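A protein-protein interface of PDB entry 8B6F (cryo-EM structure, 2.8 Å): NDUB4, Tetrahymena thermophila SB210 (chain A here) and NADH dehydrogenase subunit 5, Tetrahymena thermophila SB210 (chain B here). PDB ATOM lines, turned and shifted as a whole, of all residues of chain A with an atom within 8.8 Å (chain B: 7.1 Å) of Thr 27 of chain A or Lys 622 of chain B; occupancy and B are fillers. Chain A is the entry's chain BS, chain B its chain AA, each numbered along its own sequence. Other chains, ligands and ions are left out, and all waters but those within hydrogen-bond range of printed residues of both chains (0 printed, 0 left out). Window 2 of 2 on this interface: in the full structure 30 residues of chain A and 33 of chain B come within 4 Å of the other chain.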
ATOM      1  N   GLN A  24      -4.704  18.234  14.652  1.00  0.00           N
ATOM      2  CA  GLN A  24      -3.926  17.115  15.153  1.00  0.00           C
ATOM      3  C   GLN A  24      -3.515  16.189  14.011  1.00  0.00           C
ATOM      4  O   GLN A  24      -4.037  16.254  12.896  1.00  0.00           O
ATOM      5  CB  GLN A  24      -4.723  16.343  16.203  1.00  0.00           C
ATOM      6  CG  GLN A  24      -5.973  15.671  15.660  1.00  0.00           C
ATOM      7  CD  GLN A  24      -6.744  14.937  16.734  1.00  0.00           C
ATOM      8  OE1 GLN A  24      -6.250  14.736  17.841  1.00  0.00           O
ATOM      9  NE2 GLN A  24      -7.967  14.539  16.414  1.00  0.00           N
ATOM     10  N   ASN A  25      -2.555  15.317  14.306  1.00  0.00           N
ATOM     11  CA  ASN A  25      -2.098  14.287  13.376  1.00  0.00           C
ATOM     12  C   ASN A  25      -2.837  12.999  13.727  1.00  0.00           C
ATOM     13  O   ASN A  25      -2.480  12.305  14.682  1.00  0.00           O
ATOM     14  CB  ASN A  25      -0.585  14.114  13.469  1.00  0.00           C
ATOM     15  CG  ASN A  25      -0.051  13.106  12.476  1.00  0.00           C
ATOM     16  OD1 ASN A  25      -0.582  12.959  11.379  1.00  0.00           O
ATOM     17  ND2 ASN A  25       1.006  12.402  12.860  1.00  0.00           N
ATOM     18  N   LEU A  26      -3.874  12.680  12.950  1.00  0.00           N
ATOM     19  CA  LEU A  26      -4.730  11.547  13.279  1.00  0.00           C
ATOM     20  C   LEU A  26      -4.012  10.210  13.163  1.00  0.00           C
ATOM     21  O   LEU A  26      -4.495   9.217  13.715  1.00  0.00           O
ATOM     22  CB  LEU A  26      -5.966  11.549  12.378  1.00  0.00           C
ATOM     23  CG  LEU A  26      -6.941  12.708  12.600  1.00  0.00           C
ATOM     24  CD1 LEU A  26      -8.016  12.722  11.530  1.00  0.00           C
ATOM     25  CD2 LEU A  26      -7.575  12.625  13.977  1.00  0.00           C
ATOM     26  N   THR A  27      -2.878  10.157  12.467  1.00  0.00           N
ATOM     27  CA  THR A  27      -2.135   8.911  12.332  1.00  0.00           C
ATOM     28  C   THR A  27      -1.257   8.609  13.539  1.00  0.00           C
ATOM     29  O   THR A  27      -0.672   7.524  13.598  1.00  0.00           O
ATOM     30  CB  THR A  27      -1.268   8.943  11.072  1.00  0.00           C
ATOM     31  OG1 THR A  27      -0.373  10.061  11.126  1.00  0.00           O
ATOM     32  CG2 THR A  27      -2.137   9.049   9.829  1.00  0.00           C
ATOM     33  N   ALA A  28      -1.148   9.530  14.490  1.00  0.00           N
ATOM     34  CA  ALA A  28      -0.332   9.340  15.678  1.00  0.00           C
ATOM     35  C   ALA A  28      -1.188   8.869  16.846  1.00  0.00           C
ATOM     36  O   ALA A  28      -2.406   9.059  16.875  1.00  0.00           O
ATOM     37  CB  ALA A  28       0.390  10.638  16.051  1.00  0.00           C
ATOM     38  N   ALA A  29      -0.529   8.248  17.818  1.00  0.00           N
ATOM     39  CA  ALA A  29      -1.226   7.747  18.992  1.00  0.00           C
ATOM     40  C   ALA A  29      -1.768   8.899  19.830  1.00  0.00           C
ATOM     41  O   ALA A  29      -1.236  10.011  19.820  1.00  0.00           O
ATOM     42  CB  ALA A  29      -0.290   6.885  19.839  1.00  0.00           C
ATOM     43  N   GLN A  30      -2.845   8.622  20.560  1.00  0.00           N
ATOM     44  CA  GLN A  30      -3.429   9.633  21.430  1.00  0.00           C
ATOM     45  C   GLN A  30      -2.409  10.094  22.463  1.00  0.00           C
ATOM     46  O   GLN A  30      -1.634   9.295  22.999  1.00  0.00           O
ATOM     47  CB  GLN A  30      -4.674   9.083  22.126  1.00  0.00           C
ATOM     48  CG  GLN A  30      -5.827   8.808  21.179  1.00  0.00           C
ATOM     49  CD  GLN A  30      -7.049   8.270  21.893  1.00  0.00           C
ATOM     50  OE1 GLN A  30      -6.988   7.916  23.069  1.00  0.00           O
ATOM     51  NE2 GLN A  30      -8.170   8.210  21.185  1.00  0.00           N
ATOM     52  N   GLU A  32       0.080  12.057  21.734  1.00  0.00           N
ATOM     53  CA  GLU A  32       1.219  12.537  20.962  1.00  0.00           C
ATOM     54  C   GLU A  32       0.790  12.997  19.574  1.00  0.00           C
ATOM     55  O   GLU A  32       1.626  13.099  18.672  1.00  0.00           O
ATOM     56  CB  GLU A  32       2.295  11.452  20.860  1.00  0.00           C
ATOM     57  CG  GLU A  32       3.649  11.966  20.392  1.00  0.00           C
ATOM     58  CD  GLU A  32       4.772  10.987  20.669  1.00  0.00           C
ATOM     59  OE1 GLU A  32       4.482   9.860  21.118  1.00  0.00           O
ATOM     60  OE2 GLU A  32       5.946  11.348  20.441  1.00  0.00           O
ATOM     61  N   THR A  33      -0.498  13.272  19.387  1.00  0.00           N
ATOM     62  CA  THR A  33      -1.026  13.690  18.089  1.00  0.00           C
ATOM     63  C   THR A  33      -1.147  15.215  18.048  1.00  0.00           C
ATOM     64  O   THR A  33      -2.232  15.790  17.984  1.00  0.00           O
ATOM     65  CB  THR A  33      -2.367  13.009  17.815  1.00  0.00           C
ATOM     66  OG1 THR A  33      -2.934  13.531  16.607  1.00  0.00           O
ATOM     67  CG2 THR A  33      -3.350  13.225  18.965  1.00  0.00           C
ATOM     68  N   TYR A  34       0.013  15.865  18.088  1.00  0.00           N
ATOM     69  CA  TYR A  34       0.112  17.313  17.974  1.00  0.00           C
ATOM     70  C   TYR A  34       1.159  17.655  16.927  1.00  0.00           C
ATOM     71  O   TYR A  34       2.196  16.991  16.834  1.00  0.00           O
ATOM     72  CB  TYR A  34       0.471  17.960  19.316  1.00  0.00           C
ATOM     73  CG  TYR A  34       1.717  17.397  19.950  1.00  0.00           C
ATOM     74  CD1 TYR A  34       2.968  17.920  19.655  1.00  0.00           C
ATOM     75  CD2 TYR A  34       1.642  16.343  20.848  1.00  0.00           C
ATOM     76  CE1 TYR A  34       4.109  17.405  20.234  1.00  0.00           C
ATOM     77  CE2 TYR A  34       2.776  15.823  21.432  1.00  0.00           C
ATOM     78  CZ  TYR A  34       4.005  16.357  21.122  1.00  0.00           C
ATOM     79  OH  TYR A  34       5.137  15.838  21.705  1.00  0.00           O
ATOM     80  N   SER A  35       0.881  18.687  16.134  1.00  0.00           N
ATOM     81  CA  SER A  35       1.741  19.067  15.022  1.00  0.00           C
ATOM     82  C   SER A  35       2.568  20.315  15.278  1.00  0.00           C
ATOM     83  O   SER A  35       3.637  20.461  14.684  1.00  0.00           O
ATOM     84  CB  SER A  35       0.892  19.299  13.765  1.00  0.00           C
ATOM     85  OG  SER A  35       0.076  18.172  13.501  1.00  0.00           O
ATOM     86  N   LYS B 619       4.842  22.688   3.044  1.00  0.00           N
ATOM     87  CA  LYS B 619       4.760  21.769   1.918  1.00  0.00           C
ATOM     88  C   LYS B 619       5.594  20.509   2.101  1.00  0.00           C
ATOM     89  O   LYS B 619       5.397  19.545   1.354  1.00  0.00           O
ATOM     90  CB  LYS B 619       5.211  22.473   0.630  1.00  0.00           C
ATOM     91  CG  LYS B 619       4.341  23.656   0.236  1.00  0.00           C
ATOM     92  CD  LYS B 619       4.924  24.428  -0.940  1.00  0.00           C
ATOM     93  CE  LYS B 619       6.197  25.164  -0.549  1.00  0.00           C
ATOM     94  NZ  LYS B 619       6.699  26.040  -1.644  1.00  0.00           N
ATOM     95  N   GLY B 620       6.502  20.485   3.065  1.00  0.00           N
ATOM     96  CA  GLY B 620       7.387  19.353   3.235  1.00  0.00           C
ATOM     97  C   GLY B 620       6.693  18.155   3.850  1.00  0.00           C
ATOM     98  O   GLY B 620       5.542  18.204   4.283  1.00  0.00           O
ATOM     99  N   LYS B 621       7.430  17.048   3.886  1.00  0.00           N
ATOM    100  CA  LYS B 621       6.897  15.814   4.447  1.00  0.00           C
ATOM    101  C   LYS B 621       6.591  15.983   5.930  1.00  0.00           C
ATOM    102  O   LYS B 621       7.268  16.719   6.651  1.00  0.00           O
ATOM    103  CB  LYS B 621       7.887  14.666   4.245  1.00  0.00           C
ATOM    104  CG  LYS B 621       7.453  13.651   3.198  1.00  0.00           C
ATOM    105  CD  LYS B 621       7.348  14.272   1.816  1.00  0.00           C
ATOM    106  CE  LYS B 621       6.967  13.224   0.783  1.00  0.00           C
ATOM    107  NZ  LYS B 621       6.738  13.823  -0.560  1.00  0.00           N
ATOM    108  N   LYS B 622       5.548  15.284   6.379  1.00  0.00           N
ATOM    109  CA  LYS B 622       5.129  15.384   7.772  1.00  0.00           C
ATOM    110  C   LYS B 622       6.261  15.027   8.723  1.00  0.00           C
ATOM    111  O   LYS B 622       6.344  15.580   9.825  1.00  0.00           O
ATOM    112  CB  LYS B 622       3.926  14.473   8.013  1.00  0.00           C
ATOM    113  CG  LYS B 622       3.282  14.645   9.374  1.00  0.00           C
ATOM    114  CD  LYS B 622       2.379  13.472   9.721  1.00  0.00           C
ATOM    115  CE  LYS B 622       1.308  13.255   8.666  1.00  0.00           C
ATOM    116  NZ  LYS B 622       0.341  12.198   9.072  1.00  0.00           N
ATOM    117  N   ALA B 623       7.135  14.104   8.322  1.00  0.00           N
ATOM    118  CA  ALA B 623       8.206  13.662   9.209  1.00  0.00           C
ATOM    119  C   ALA B 623       9.149  14.807   9.552  1.00  0.00           C
ATOM    120  O   ALA B 623       9.588  14.936  10.699  1.00  0.00           O
ATOM    121  CB  ALA B 623       8.976  12.511   8.565  1.00  0.00           C
ATOM    122  N   ILE B 624       9.475  15.648   8.571  1.00  0.00           N
ATOM    123  CA  ILE B 624      10.438  16.721   8.807  1.00  0.00           C
ATOM    124  C   ILE B 624      10.001  17.576   9.988  1.00  0.00           C
ATOM    125  O   ILE B 624      10.815  17.940  10.846  1.00  0.00           O
ATOM    126  CB  ILE B 624      10.615  17.572   7.535  1.00  0.00           C
ATOM    127  CG1 ILE B 624      10.988  16.699   6.333  1.00  0.00           C
ATOM    128  CG2 ILE B 624      11.676  18.643   7.751  1.00  0.00           C
ATOM    129  CD1 ILE B 624      12.221  15.856   6.526  1.00  0.00           C
ATOM    130  N   TYR B 625       8.711  17.907  10.058  1.00  0.00           N
ATOM    131  CA  TYR B 625       8.218  18.758  11.133  1.00  0.00           C
ATOM    132  C   TYR B 625       7.990  17.978  12.423  1.00  0.00           C
ATOM    133  O   TYR B 625       8.332  18.459  13.508  1.00  0.00           O
ATOM    134  CB  TYR B 625       6.923  19.441  10.698  1.00  0.00           C
ATOM    135  CG  TYR B 625       7.040  20.177   9.388  1.00  0.00           C
ATOM    136  CD1 TYR B 625       7.565  21.460   9.341  1.00  0.00           C
ATOM    137  CD2 TYR B 625       6.624  19.594   8.200  1.00  0.00           C
ATOM    138  CE1 TYR B 625       7.674  22.142   8.152  1.00  0.00           C
ATOM    139  CE2 TYR B 625       6.731  20.269   7.001  1.00  0.00           C
ATOM    140  CZ  TYR B 625       7.257  21.544   6.986  1.00  0.00           C
ATOM    141  OH  TYR B 625       7.369  22.230   5.803  1.00  0.00           O
ATOM    142  N   LEU B 626       7.416  16.779  12.329  1.00  0.00           N
ATOM    143  CA  LEU B 626       7.075  16.032  13.535  1.00  0.00           C
ATOM    144  C   LEU B 626       8.322  15.603  14.296  1.00  0.00           C
ATOM    145  O   LEU B 626       8.358  15.681  15.529  1.00  0.00           O
ATOM    146  CB  LEU B 626       6.220  14.818  13.178  1.00  0.00           C
ATOM    147  CG  LEU B 626       4.711  15.054  13.242  1.00  0.00           C
ATOM    148  CD1 LEU B 626       4.302  16.279  12.433  1.00  0.00           C
ATOM    149  CD2 LEU B 626       3.964  13.815  12.779  1.00  0.00           C
ATOM    150  N   GLN B 627       9.355  15.154  13.582  1.00  0.00           N
ATOM    151  CA  GLN B 627      10.560  14.682  14.253  1.00  0.00           C
ATOM    152  C   GLN B 627      11.186  15.770  15.112  1.00  0.00           C
ATOM    153  O   GLN B 627      11.875  15.464  16.092  1.00  0.00           O
ATOM    154  CB  GLN B 627      11.570  14.178  13.222  1.00  0.00           C
ATOM    155  CG  GLN B 627      11.081  13.006  12.381  1.00  0.00           C
ATOM    156  CD  GLN B 627      10.997  11.720  13.168  1.00  0.00           C
ATOM    157  OE1 GLN B 627      11.408  11.657  14.325  1.00  0.00           O
ATOM    158  NE2 GLN B 627      10.461  10.680  12.540  1.00  0.00           N
ATOM    159  N   ALA B 628      10.964  17.037  14.767  1.00  0.00           N
ATOM    160  CA  ALA B 628      11.542  18.154  15.499  1.00  0.00           C
ATOM    161  C   ALA B 628      10.560  18.845  16.435  1.00  0.00           C
ATOM    162  O   ALA B 628      10.992  19.642  17.274  1.00  0.00           O
ATOM    163  CB  ALA B 628      12.106  19.187  14.516  1.00  0.00           C
ATOM    164  N   SER B 629       9.262  18.577  16.310  1.00  0.00           N
ATOM    165  CA  SER B 629       8.256  19.205  17.157  1.00  0.00           C
ATOM    166  C   SER B 629       7.976  18.437  18.445  1.00  0.00           C
ATOM    167  O   SER B 629       7.101  18.852  19.210  1.00  0.00           O
ATOM    168  CB  SER B 629       6.949  19.378  16.377  1.00  0.00           C
ATOM    169  OG  SER B 629       6.408  18.125  16.001  1.00  0.00           O
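The side-chain amino group (NZ) of Lys 622 of chain B lies within hydrogen-bond range of the side-chain amide oxygen (OD1) of Asn 25 of chain A (2.6 Å).
NZ of Lys 622 of chain B lies within hydrogen-bond range of OG1 of Thr 27 of chain A (3.0 Å).
The backbone NH of Asn 25 of chain A lies close to the side-chain hydroxyl of Thr 33 of chain A.
OG1 of Thr 27 of chain A lies within hydrogen-bond range of OD1 of Asn 25 of chain A, at 2.9 Å.
The backbone carbonyl oxygen of Leu 626 of chain B lies within hydrogen-bond range of the side-chain hydroxyl of Ser 629 of chain B, at 3.2 Å.
OG of Ser 629 of chain B is in hydrogen-bond range of O of Tyr 625 of chain B.
Among the printed residues, pairs that only touch across the chains: Asn 25 of chain A with Leu 626 of chain B (3.3 Å), Tyr 34 of chain A with Ser 629 of chain B (3.5 Å) and Ser 35 of chain A with Ser 629 of chain B (3.9 Å).
Thr 27 of chain A touches just one residue of chain B: Lys 622 (3.0 Å).
Lys 622 of chain B touches just these residues of chain A: Asn 25 (2.6 Å) and Thr 27 (3.0 Å).
Of the printed residues of chain A, Ser 629 of chain B touches Tyr 34 (3.5 Å) and Ser 35 (3.9 Å).
Printed residues of chain B within 4 Å of Asn 25 of chain A: Lys 622 (2.6 Å) and Leu 626 (3.3 Å).
The nearest residue of chain B that does not touch Thr 27 of chain A is Leu 626 of chain B (6.0 Å).
The nearest printed residue of chain A that does not touch Ser 629 of chain B is Glu 32 of chain A (7.4 Å).
Hydrophobic or aromatic side chains of chain B that line the printed part of chain A: Leu 626.
Along chain B the printed residues that touch a printed residue of chain A span positions 622 to 629.
Hydrophobic or aromatic side chains of chain A within 4 Å of the printed part of chain B: Tyr 34.
Among the printed residues, no Asp or Glu carboxylate lies within 4 Å of a Lys or Arg side-chain nitrogen of the other chain.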
